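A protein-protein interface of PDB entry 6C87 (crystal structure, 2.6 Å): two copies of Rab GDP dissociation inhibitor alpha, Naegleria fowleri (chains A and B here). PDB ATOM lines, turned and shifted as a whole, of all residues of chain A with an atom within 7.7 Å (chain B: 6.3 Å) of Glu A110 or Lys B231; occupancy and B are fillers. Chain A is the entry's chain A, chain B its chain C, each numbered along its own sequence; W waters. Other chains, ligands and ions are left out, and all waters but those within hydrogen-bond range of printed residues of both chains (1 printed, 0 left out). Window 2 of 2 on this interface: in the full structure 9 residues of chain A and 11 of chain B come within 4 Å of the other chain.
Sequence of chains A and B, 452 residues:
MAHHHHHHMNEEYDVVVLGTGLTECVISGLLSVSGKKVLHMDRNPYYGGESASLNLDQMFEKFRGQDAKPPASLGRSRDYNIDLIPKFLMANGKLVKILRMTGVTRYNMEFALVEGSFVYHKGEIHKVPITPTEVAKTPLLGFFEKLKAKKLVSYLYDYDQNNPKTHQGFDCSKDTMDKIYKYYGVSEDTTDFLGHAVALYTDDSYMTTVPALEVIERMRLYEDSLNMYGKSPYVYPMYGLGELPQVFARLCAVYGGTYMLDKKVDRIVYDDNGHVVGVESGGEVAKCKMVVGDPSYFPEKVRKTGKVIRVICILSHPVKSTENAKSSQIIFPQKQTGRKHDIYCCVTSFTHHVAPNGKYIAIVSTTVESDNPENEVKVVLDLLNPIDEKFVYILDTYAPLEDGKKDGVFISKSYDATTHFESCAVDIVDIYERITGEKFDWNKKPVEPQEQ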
ATOM      1  N   VAL A 104      -6.505  16.634 -40.220  1.00  0.00           N
ATOM      2  CA  VAL A 104      -5.938  17.035 -38.938  1.00  0.00           C
ATOM      3  C   VAL A 104      -6.969  16.976 -37.819  1.00  0.00           C
ATOM      4  O   VAL A 104      -6.591  16.872 -36.646  1.00  0.00           O
ATOM      5  CB  VAL A 104      -5.347  18.458 -39.002  1.00  0.00           C
ATOM      6  CG1 VAL A 104      -4.182  18.508 -39.960  1.00  0.00           C
ATOM      7  CG2 VAL A 104      -6.426  19.481 -39.365  1.00  0.00           C
ATOM      8  N   THR A 105      -8.267  17.032 -38.150  1.00  0.00           N
ATOM      9  CA  THR A 105      -9.318  17.004 -37.135  1.00  0.00           C
ATOM     10  C   THR A 105      -9.462  15.641 -36.472  1.00  0.00           C
ATOM     11  O   THR A 105     -10.022  15.563 -35.372  1.00  0.00           O
ATOM     12  CB  THR A 105     -10.665  17.431 -37.738  1.00  0.00           C
ATOM     13  OG1 THR A 105     -10.925  16.694 -38.942  1.00  0.00           O
ATOM     14  CG2 THR A 105     -10.689  18.922 -38.030  1.00  0.00           C
ATOM     15  N   ARG A 106      -8.972  14.574 -37.111  1.00  0.00           N
ATOM     16  CA  ARG A 106      -9.028  13.228 -36.549  1.00  0.00           C
ATOM     17  C   ARG A 106      -7.913  12.950 -35.547  1.00  0.00           C
ATOM     18  O   ARG A 106      -7.926  11.892 -34.907  1.00  0.00           O
ATOM     19  CB  ARG A 106      -8.980  12.189 -37.675  1.00  0.00           C
ATOM     20  CG  ARG A 106     -10.343  11.650 -38.070  1.00  0.00           C
ATOM     21  CD  ARG A 106     -10.348  11.060 -39.469  1.00  0.00           C
ATOM     22  NE  ARG A 106     -11.678  10.580 -39.839  1.00  0.00           N
ATOM     23  CZ  ARG A 106     -12.650  11.349 -40.323  1.00  0.00           C
ATOM     24  NH1 ARG A 106     -12.448  12.649 -40.499  1.00  0.00           N
ATOM     25  NH2 ARG A 106     -13.828  10.820 -40.629  1.00  0.00           N
ATOM     26  N   TYR A 107      -6.966  13.874 -35.385  1.00  0.00           N
ATOM     27  CA  TYR A 107      -5.850  13.717 -34.457  1.00  0.00           C
ATOM     28  C   TYR A 107      -6.328  13.824 -33.014  1.00  0.00           C
ATOM     29  O   TYR A 107      -7.532  13.744 -32.748  1.00  0.00           O
ATOM     30  CB  TYR A 107      -4.768  14.763 -34.739  1.00  0.00           C
ATOM     31  CG  TYR A 107      -3.998  14.532 -36.026  1.00  0.00           C
ATOM     32  CD1 TYR A 107      -2.802  15.192 -36.267  1.00  0.00           C
ATOM     33  CD2 TYR A 107      -4.466  13.657 -37.001  1.00  0.00           C
ATOM     34  CE1 TYR A 107      -2.088  14.982 -37.440  1.00  0.00           C
ATOM     35  CE2 TYR A 107      -3.762  13.442 -38.177  1.00  0.00           C
ATOM     36  CZ  TYR A 107      -2.573  14.107 -38.390  1.00  0.00           C
ATOM     37  OH  TYR A 107      -1.868  13.897 -39.555  1.00  0.00           O
ATOM     38  N   ASN A 108      -5.403  14.031 -32.074  1.00  0.00           N
ATOM     39  CA  ASN A 108      -5.769  14.212 -30.669  1.00  0.00           C
ATOM     40  C   ASN A 108      -6.227  15.656 -30.450  1.00  0.00           C
ATOM     41  O   ASN A 108      -5.651  16.436 -29.693  1.00  0.00           O
ATOM     42  CB  ASN A 108      -4.600  13.846 -29.762  1.00  0.00           C
ATOM     43  N   MET A 109      -7.305  15.993 -31.154  1.00  0.00           N
ATOM     44  CA  MET A 109      -7.839  17.345 -31.206  1.00  0.00           C
ATOM     45  C   MET A 109      -9.328  17.330 -30.894  1.00  0.00           C
ATOM     46  O   MET A 109     -10.086  16.583 -31.519  1.00  0.00           O
ATOM     47  CB  MET A 109      -7.588  17.956 -32.586  1.00  0.00           C
ATOM     48  CG  MET A 109      -8.111  19.351 -32.736  1.00  0.00           C
ATOM     49  SD  MET A 109      -7.424  20.146 -34.193  1.00  0.00           S
ATOM     50  CE  MET A 109      -7.363  21.824 -33.588  1.00  0.00           C
ATOM     51  N   GLU A 110      -9.736  18.115 -29.903  1.00  0.00           N
ATOM     52  CA  GLU A 110     -11.123  18.200 -29.472  1.00  0.00           C
ATOM     53  C   GLU A 110     -11.690  19.589 -29.751  1.00  0.00           C
ATOM     54  O   GLU A 110     -11.096  20.599 -29.358  1.00  0.00           O
ATOM     55  CB  GLU A 110     -11.268  17.880 -27.985  1.00  0.00           C
ATOM     56  CG  GLU A 110     -12.700  18.053 -27.498  1.00  0.00           C
ATOM     57  CD  GLU A 110     -12.858  17.822 -26.013  1.00  0.00           C
ATOM     58  OE1 GLU A 110     -11.872  17.401 -25.364  1.00  0.00           O
ATOM     59  OE2 GLU A 110     -13.970  18.080 -25.495  1.00  0.00           O
ATOM     60  N   PHE A 111     -12.858  19.636 -30.388  1.00  0.00           N
ATOM     61  CA  PHE A 111     -13.613  20.873 -30.533  1.00  0.00           C
ATOM     62  C   PHE A 111     -14.683  20.912 -29.451  1.00  0.00           C
ATOM     63  O   PHE A 111     -15.406  19.931 -29.246  1.00  0.00           O
ATOM     64  CB  PHE A 111     -14.249  20.986 -31.921  1.00  0.00           C
ATOM     65  CG  PHE A 111     -13.263  21.284 -33.010  1.00  0.00           C
ATOM     66  CD1 PHE A 111     -12.661  22.526 -33.093  1.00  0.00           C
ATOM     67  CD2 PHE A 111     -12.928  20.322 -33.949  1.00  0.00           C
ATOM     68  CE1 PHE A 111     -11.742  22.808 -34.097  1.00  0.00           C
ATOM     69  CE2 PHE A 111     -12.008  20.598 -34.954  1.00  0.00           C
ATOM     70  CZ  PHE A 111     -11.414  21.841 -35.027  1.00  0.00           C
ATOM     71  N   ALA A 112     -14.771  22.045 -28.756  1.00  0.00           N
ATOM     72  CA  ALA A 112     -15.748  22.262 -27.701  1.00  0.00           C
ATOM     73  C   ALA A 112     -16.685  23.401 -28.072  1.00  0.00           C
ATOM     74  O   ALA A 112     -16.301  24.336 -28.786  1.00  0.00           O
ATOM     75  CB  ALA A 112     -15.059  22.567 -26.373  1.00  0.00           C
ATOM     76  N   LEU A 113     -17.920  23.316 -27.584  1.00  0.00           N
ATOM     77  CA  LEU A 113     -18.937  24.284 -27.973  1.00  0.00           C
ATOM     78  C   LEU A 113     -18.754  25.611 -27.238  1.00  0.00           C
ATOM     79  O   LEU A 113     -18.178  25.682 -26.147  1.00  0.00           O
ATOM     80  CB  LEU A 113     -20.337  23.712 -27.736  1.00  0.00           C
ATOM     81  CG  LEU A 113     -20.771  23.195 -26.358  1.00  0.00           C
ATOM     82  CD1 LEU A 113     -21.411  24.321 -25.537  1.00  0.00           C
ATOM     83  CD2 LEU A 113     -21.666  21.940 -26.431  1.00  0.00           C
ATOM     84  N   VAL A 235     -17.996  26.463 -32.398  1.00  0.00           N
ATOM     85  CA  VAL A 235     -17.053  25.633 -31.660  1.00  0.00           C
ATOM     86  C   VAL A 235     -15.693  26.334 -31.658  1.00  0.00           C
ATOM     87  O   VAL A 235     -15.433  27.251 -32.441  1.00  0.00           O
ATOM     88  CB  VAL A 235     -16.928  24.211 -32.248  1.00  0.00           C
ATOM     89  CG1 VAL A 235     -18.283  23.523 -32.294  1.00  0.00           C
ATOM     90  CG2 VAL A 235     -16.266  24.239 -33.616  1.00  0.00           C
ATOM     91  N   TYR A 236     -14.806  25.850 -30.785  1.00  0.00           N
ATOM     92  CA  TYR A 236     -13.464  26.396 -30.538  1.00  0.00           C
ATOM     93  C   TYR A 236     -12.619  25.223 -30.072  1.00  0.00           C
ATOM     94  O   TYR A 236     -13.127  24.363 -29.335  1.00  0.00           O
ATOM     95  CB  TYR A 236     -13.468  27.496 -29.470  1.00  0.00           C
ATOM     96  CG  TYR A 236     -12.238  28.391 -29.393  1.00  0.00           C
ATOM     97  CD1 TYR A 236     -11.928  29.270 -30.423  1.00  0.00           C
ATOM     98  CD2 TYR A 236     -11.420  28.393 -28.265  1.00  0.00           C
ATOM     99  CE1 TYR A 236     -10.825  30.110 -30.345  1.00  0.00           C
ATOM    100  CE2 TYR A 236     -10.312  29.232 -28.174  1.00  0.00           C
ATOM    101  CZ  TYR A 236     -10.024  30.092 -29.220  1.00  0.00           C
ATOM    102  OH  TYR A 236      -8.930  30.933 -29.164  1.00  0.00           O
ATOM    103  N   PRO A 237     -11.350  25.146 -30.466  1.00  0.00           N
ATOM    104  CA  PRO A 237     -10.544  23.990 -30.064  1.00  0.00           C
ATOM    105  C   PRO A 237     -10.166  24.074 -28.595  1.00  0.00           C
ATOM    106  O   PRO A 237      -9.892  25.151 -28.059  1.00  0.00           O
ATOM    107  CB  PRO A 237      -9.305  24.075 -30.968  1.00  0.00           C
ATOM    108  CG  PRO A 237      -9.568  25.211 -31.931  1.00  0.00           C
ATOM    109  CD  PRO A 237     -10.581  26.093 -31.289  1.00  0.00           C
ATOM    110  N   MET A 238     -10.175  22.917 -27.943  1.00  0.00           N
ATOM    111  CA  MET A 238      -9.655  22.804 -26.588  1.00  0.00           C
ATOM    112  C   MET A 238      -8.182  23.215 -26.578  1.00  0.00           C
ATOM    113  O   MET A 238      -7.394  22.776 -27.426  1.00  0.00           O
ATOM    114  CB  MET A 238      -9.836  21.363 -26.090  1.00  0.00           C
ATOM    115  CG  MET A 238     -10.016  21.222 -24.588  1.00  0.00           C
ATOM    116  SD  MET A 238     -11.542  21.985 -23.982  1.00  0.00           S
ATOM    117  CE  MET A 238     -12.744  20.788 -24.510  1.00  0.00           C
ATOM    118  N   TYR A 239      -7.818  24.071 -25.623  1.00  0.00           N
ATOM    119  CA  TYR A 239      -6.506  24.705 -25.489  1.00  0.00           C
ATOM    120  C   TYR A 239      -6.269  25.789 -26.534  1.00  0.00           C
ATOM    121  O   TYR A 239      -5.183  26.388 -26.553  1.00  0.00           O
ATOM    122  CB  TYR A 239      -5.350  23.684 -25.514  1.00  0.00           C
ATOM    123  CG  TYR A 239      -5.493  22.613 -24.455  1.00  0.00           C
ATOM    124  CD1 TYR A 239      -5.080  22.849 -23.147  1.00  0.00           C
ATOM    125  CD2 TYR A 239      -6.083  21.384 -24.746  1.00  0.00           C
ATOM    126  CE1 TYR A 239      -5.223  21.882 -22.165  1.00  0.00           C
ATOM    127  CE2 TYR A 239      -6.228  20.409 -23.770  1.00  0.00           C
ATOM    128  CZ  TYR A 239      -5.801  20.668 -22.485  1.00  0.00           C
ATOM    129  OH  TYR A 239      -5.948  19.707 -21.513  1.00  0.00           O
ATOM    130  N   GLY A 240      -7.246  26.084 -27.385  1.00  0.00           N
ATOM    131  CA  GLY A 240      -7.157  27.233 -28.262  1.00  0.00           C
ATOM    132  C   GLY A 240      -6.518  26.929 -29.598  1.00  0.00           C
ATOM    133  O   GLY A 240      -6.056  25.818 -29.879  1.00  0.00           O
ATOM    134  N   GLU A 243      -3.325  24.888 -31.062  1.00  0.00           N
ATOM    135  CA  GLU A 243      -3.291  23.465 -31.366  1.00  0.00           C
ATOM    136  C   GLU A 243      -3.199  23.209 -32.861  1.00  0.00           C
ATOM    137  O   GLU A 243      -2.614  22.205 -33.278  1.00  0.00           O
ATOM    138  CB  GLU A 243      -4.546  22.796 -30.801  1.00  0.00           C
ATOM    139  CG  GLU A 243      -4.643  22.867 -29.298  1.00  0.00           C
ATOM    140  CD  GLU A 243      -3.648  21.950 -28.624  1.00  0.00           C
ATOM    141  OE1 GLU A 243      -3.871  20.716 -28.651  1.00  0.00           O
ATOM    142  OE2 GLU A 243      -2.630  22.460 -28.103  1.00  0.00           O
ATOM    143  N   THR A 351     -13.051  26.837 -19.534  1.00  0.00           N
ATOM    144  CA  THR A 351     -13.800  25.762 -20.180  1.00  0.00           C
ATOM    145  C   THR A 351     -13.181  25.333 -21.500  1.00  0.00           C
ATOM    146  O   THR A 351     -13.451  24.218 -21.961  1.00  0.00           O
ATOM    147  CB  THR A 351     -15.273  26.147 -20.408  1.00  0.00           C
ATOM    148  OG1 THR A 351     -15.368  27.366 -21.158  1.00  0.00           O
ATOM    149  CG2 THR A 351     -16.013  26.271 -19.090  1.00  0.00           C
ATOM    150  N   HIS A 352     -12.364  26.183 -22.118  1.00  0.00           N
ATOM    151  CA  HIS A 352     -11.569  25.775 -23.265  1.00  0.00           C
ATOM    152  C   HIS A 352     -10.093  25.634 -22.916  1.00  0.00           C
ATOM    153  O   HIS A 352      -9.264  25.465 -23.816  1.00  0.00           O
ATOM    154  CB  HIS A 352     -11.769  26.760 -24.417  1.00  0.00           C
ATOM    155  CG  HIS A 352     -13.106  26.634 -25.085  1.00  0.00           C
ATOM    156  ND1 HIS A 352     -14.202  27.384 -24.709  1.00  0.00           N
ATOM    157  CD2 HIS A 352     -13.537  25.803 -26.065  1.00  0.00           C
ATOM    158  CE1 HIS A 352     -15.238  27.049 -25.459  1.00  0.00           C
ATOM    159  NE2 HIS A 352     -14.863  26.088 -26.285  1.00  0.00           N
ATOM    160  N   HIS A 353      -9.760  25.661 -21.619  1.00  0.00           N
ATOM    161  CA  HIS A 353      -8.386  25.555 -21.123  1.00  0.00           C
ATOM    162  C   HIS A 353      -7.472  26.598 -21.758  1.00  0.00           C
ATOM    163  O   HIS A 353      -6.348  26.304 -22.170  1.00  0.00           O
ATOM    164  CB  HIS A 353      -7.815  24.154 -21.325  1.00  0.00           C
ATOM    165  CG  HIS A 353      -8.373  23.147 -20.380  1.00  0.00           C
ATOM    166  ND1 HIS A 353      -9.343  22.242 -20.747  1.00  0.00           N
ATOM    167  CD2 HIS A 353      -8.145  22.943 -19.063  1.00  0.00           C
ATOM    168  CE1 HIS A 353      -9.661  21.495 -19.704  1.00  0.00           C
ATOM    169  NE2 HIS A 353      -8.953  21.907 -18.667  1.00  0.00           N
ATOM    170  N   ALA B 112     -19.378  14.588 -22.516  1.00  0.00           N
ATOM    171  CA  ALA B 112     -17.979  14.586 -22.894  1.00  0.00           C
ATOM    172  C   ALA B 112     -17.735  13.423 -23.839  1.00  0.00           C
ATOM    173  O   ALA B 112     -18.379  12.372 -23.740  1.00  0.00           O
ATOM    174  CB  ALA B 112     -17.063  14.479 -21.671  1.00  0.00           C
ATOM    175  N   LEU B 113     -16.802  13.615 -24.760  1.00  0.00           N
ATOM    176  CA  LEU B 113     -16.572  12.578 -25.744  1.00  0.00           C
ATOM    177  C   LEU B 113     -15.771  11.428 -25.136  1.00  0.00           C
ATOM    178  O   LEU B 113     -15.029  11.583 -24.164  1.00  0.00           O
ATOM    179  CB  LEU B 113     -15.869  13.142 -26.982  1.00  0.00           C
ATOM    180  CG  LEU B 113     -14.582  13.926 -26.784  1.00  0.00           C
ATOM    181  CD1 LEU B 113     -13.398  12.990 -26.699  1.00  0.00           C
ATOM    182  CD2 LEU B 113     -14.404  14.899 -27.929  1.00  0.00           C
ATOM    183  N   VAL B 114     -15.929  10.282 -25.733  1.00  0.00           N
ATOM    184  CA  VAL B 114     -15.140   9.105 -25.417  1.00  0.00           C
ATOM    185  C   VAL B 114     -13.878   9.171 -26.264  1.00  0.00           C
ATOM    186  O   VAL B 114     -13.918   9.606 -27.420  1.00  0.00           O
ATOM    187  CB  VAL B 114     -15.972   7.834 -25.683  1.00  0.00           C
ATOM    188  CG1 VAL B 114     -15.156   6.570 -25.485  1.00  0.00           C
ATOM    189  CG2 VAL B 114     -17.207   7.822 -24.769  1.00  0.00           C
ATOM    190  N   GLU B 115     -12.736   8.797 -25.686  1.00  0.00           N
ATOM    191  CA  GLU B 115     -11.485   9.056 -26.392  1.00  0.00           C
ATOM    192  C   GLU B 115     -11.169   8.001 -27.437  1.00  0.00           C
ATOM    193  O   GLU B 115     -10.584   8.330 -28.475  1.00  0.00           O
ATOM    194  CB  GLU B 115     -10.312   9.130 -25.411  1.00  0.00           C
ATOM    195  CG  GLU B 115     -10.288  10.338 -24.501  1.00  0.00           C
ATOM    196  CD  GLU B 115      -9.217  10.216 -23.423  1.00  0.00           C
ATOM    197  OE1 GLU B 115      -8.218   9.486 -23.622  1.00  0.00           O
ATOM    198  OE2 GLU B 115      -9.380  10.856 -22.369  1.00  0.00           O
ATOM    199  N   GLY B 116     -11.581   6.760 -27.220  1.00  0.00           N
ATOM    200  CA  GLY B 116     -11.132   5.665 -28.051  1.00  0.00           C
ATOM    201  C   GLY B 116     -12.267   4.787 -28.533  1.00  0.00           C
ATOM    202  O   GLY B 116     -13.257   4.569 -27.835  1.00  0.00           O
ATOM    203  N   SER B 117     -12.078   4.248 -29.737  1.00  0.00           N
ATOM    204  CA  SER B 117     -12.989   3.282 -30.342  1.00  0.00           C
ATOM    205  C   SER B 117     -12.161   2.136 -30.903  1.00  0.00           C
ATOM    206  O   SER B 117     -11.439   2.310 -31.890  1.00  0.00           O
ATOM    207  CB  SER B 117     -13.834   3.922 -31.441  1.00  0.00           C
ATOM    208  OG  SER B 117     -14.721   2.964 -31.984  1.00  0.00           O
ATOM    209  N   LEU B 226     -18.276  11.218 -35.384  1.00  0.00           N
ATOM    210  CA  LEU B 226     -16.856  11.444 -35.146  1.00  0.00           C
ATOM    211  C   LEU B 226     -16.442  12.866 -35.518  1.00  0.00           C
ATOM    212  O   LEU B 226     -15.585  13.468 -34.858  1.00  0.00           O
ATOM    213  CB  LEU B 226     -16.049  10.409 -35.922  1.00  0.00           C
ATOM    214  CG  LEU B 226     -14.546  10.605 -36.056  1.00  0.00           C
ATOM    215  CD1 LEU B 226     -13.865  10.357 -34.732  1.00  0.00           C
ATOM    216  CD2 LEU B 226     -14.036   9.657 -37.114  1.00  0.00           C
ATOM    217  N   TYR B 229     -17.102  16.391 -32.608  1.00  0.00           N
ATOM    218  CA  TYR B 229     -16.146  16.884 -31.628  1.00  0.00           C
ATOM    219  C   TYR B 229     -14.749  16.323 -31.820  1.00  0.00           C
ATOM    220  O   TYR B 229     -13.782  16.962 -31.398  1.00  0.00           O
ATOM    221  CB  TYR B 229     -16.608  16.526 -30.205  1.00  0.00           C
ATOM    222  CG  TYR B 229     -18.057  16.854 -29.949  1.00  0.00           C
ATOM    223  CD1 TYR B 229     -18.518  18.166 -29.942  1.00  0.00           C
ATOM    224  CD2 TYR B 229     -18.972  15.837 -29.742  1.00  0.00           C
ATOM    225  CE1 TYR B 229     -19.854  18.444 -29.724  1.00  0.00           C
ATOM    226  CE2 TYR B 229     -20.295  16.104 -29.527  1.00  0.00           C
ATOM    227  CZ  TYR B 229     -20.736  17.402 -29.516  1.00  0.00           C
ATOM    228  OH  TYR B 229     -22.072  17.641 -29.298  1.00  0.00           O
ATOM    229  N   GLY B 230     -14.618  15.177 -32.479  1.00  0.00           N
ATOM    230  CA  GLY B 230     -13.348  14.535 -32.733  1.00  0.00           C
ATOM    231  C   GLY B 230     -13.127  13.342 -31.815  1.00  0.00           C
ATOM    232  O   GLY B 230     -13.909  13.056 -30.905  1.00  0.00           O
ATOM    233  N   LYS B 231     -12.044  12.615 -32.118  1.00  0.00           N
ATOM    234  CA  LYS B 231     -11.536  11.455 -31.382  1.00  0.00           C
ATOM    235  C   LYS B 231     -12.353  10.163 -31.512  1.00  0.00           C
ATOM    236  O   LYS B 231     -11.773   9.101 -31.762  1.00  0.00           O
ATOM    237  CB  LYS B 231     -11.381  11.825 -29.901  1.00  0.00           C
ATOM    238  CG  LYS B 231     -10.146  12.670 -29.589  1.00  0.00           C
ATOM    239  CD  LYS B 231     -10.417  13.567 -28.395  1.00  0.00           C
ATOM    240  CE  LYS B 231      -9.158  13.997 -27.673  1.00  0.00           C
ATOM    241  NZ  LYS B 231      -9.515  14.641 -26.370  1.00  0.00           N
ATOM    242  N   SER B 232     -13.672  10.214 -31.356  1.00  0.00           N
ATOM    243  CA  SER B 232     -14.500   9.018 -31.471  1.00  0.00           C
ATOM    244  C   SER B 232     -15.930   9.466 -31.728  1.00  0.00           C
ATOM    245  O   SER B 232     -16.257  10.650 -31.562  1.00  0.00           O
ATOM    246  CB  SER B 232     -14.413   8.130 -30.213  1.00  0.00           C
ATOM    247  OG  SER B 232     -15.421   8.438 -29.271  1.00  0.00           O
ATOM    248  N   PRO B 233     -16.812   8.553 -32.134  1.00  0.00           N
ATOM    249  CA  PRO B 233     -18.208   8.943 -32.363  1.00  0.00           C
ATOM    250  C   PRO B 233     -19.052   8.952 -31.104  1.00  0.00           C
ATOM    251  O   PRO B 233     -20.250   9.243 -31.179  1.00  0.00           O
ATOM    252  CB  PRO B 233     -18.701   7.865 -33.344  1.00  0.00           C
ATOM    253  CG  PRO B 233     -17.939   6.647 -32.931  1.00  0.00           C
ATOM    254  CD  PRO B 233     -16.562   7.153 -32.533  1.00  0.00           C
HETATM  255  O   HOH W   1      -8.824  17.551 -25.629  1.00  0.00           O
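The side-chain carboxylate (OE1) of Glu A110 lies within salt-bridge range of the side-chain amino group (NZ) of Lys B231 (3.8 Å). The backbone NH (N) of Phe A111 lies within hydrogen-bond range of the backbone carbonyl oxygen (O) of Tyr B229 (3.0 Å).
The backbone NH (N) of Met A238 is in hydrogen-bond range of the backbone carbonyl oxygen (O) of Glu A110, at 2.9 Å.
Arg A106 touches Leu B226 (NH2 to CD2, 3.7 Å). Tyr B229 touches Met A109 (O to O, 3.7 Å). Leu B113 touches Glu A110 (CD2 to CG, 3.6 Å). O of Tyr B229 touches CA of Glu A110 (3.5 Å).
Of the printed residues of chain B, Met A109 touches Tyr B229. Of the printed residues of chain B, Phe A111 touches Tyr B229. Leu A113 touches none of the printed residues of chain B. Of the printed residues of chain A, Leu B113 touches Glu A110. Ser B117 touches none of the printed residues of chain A. Printed residues of chain A within 4 Å of Tyr B229: Met A109, Glu A110 and Phe A111. No residue of chain A comes within 4 Å of Gly B230. Of chain A, only Glu A110 (3.8 Å) comes within 4 Å of Lys B231. The nearest residue of chain B that does not touch Glu A110 is Gly B230 (5.4 Å).
Of the 12 printed residues of chain B, 4 touch a printed residue of chain A. Hydrophobic or aromatic side chains of chain B within 4 Å of the printed part of chain A: Leu B113, Leu B226 and Tyr B229. Of the 20 printed residues of chain A, 4 touch a printed residue of chain B. Printed residues of chain A that touch a printed residue of chain B: Arg A106, Met A109, Glu A110 and Phe A111. Among the printed residues, 6 pairs touch across the chains. Among the printed residues, Asp or Glu carboxylates within 4 Å of a Lys or Arg side-chain nitrogen of the other chain: Glu A110 with Lys B231 (3.8 Å).
Positions printed for both chains: 112 and 113.
Water W1 bridges OE1 of Glu A110 (3.1 Å) and NZ of Lys B231 (3.1 Å).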
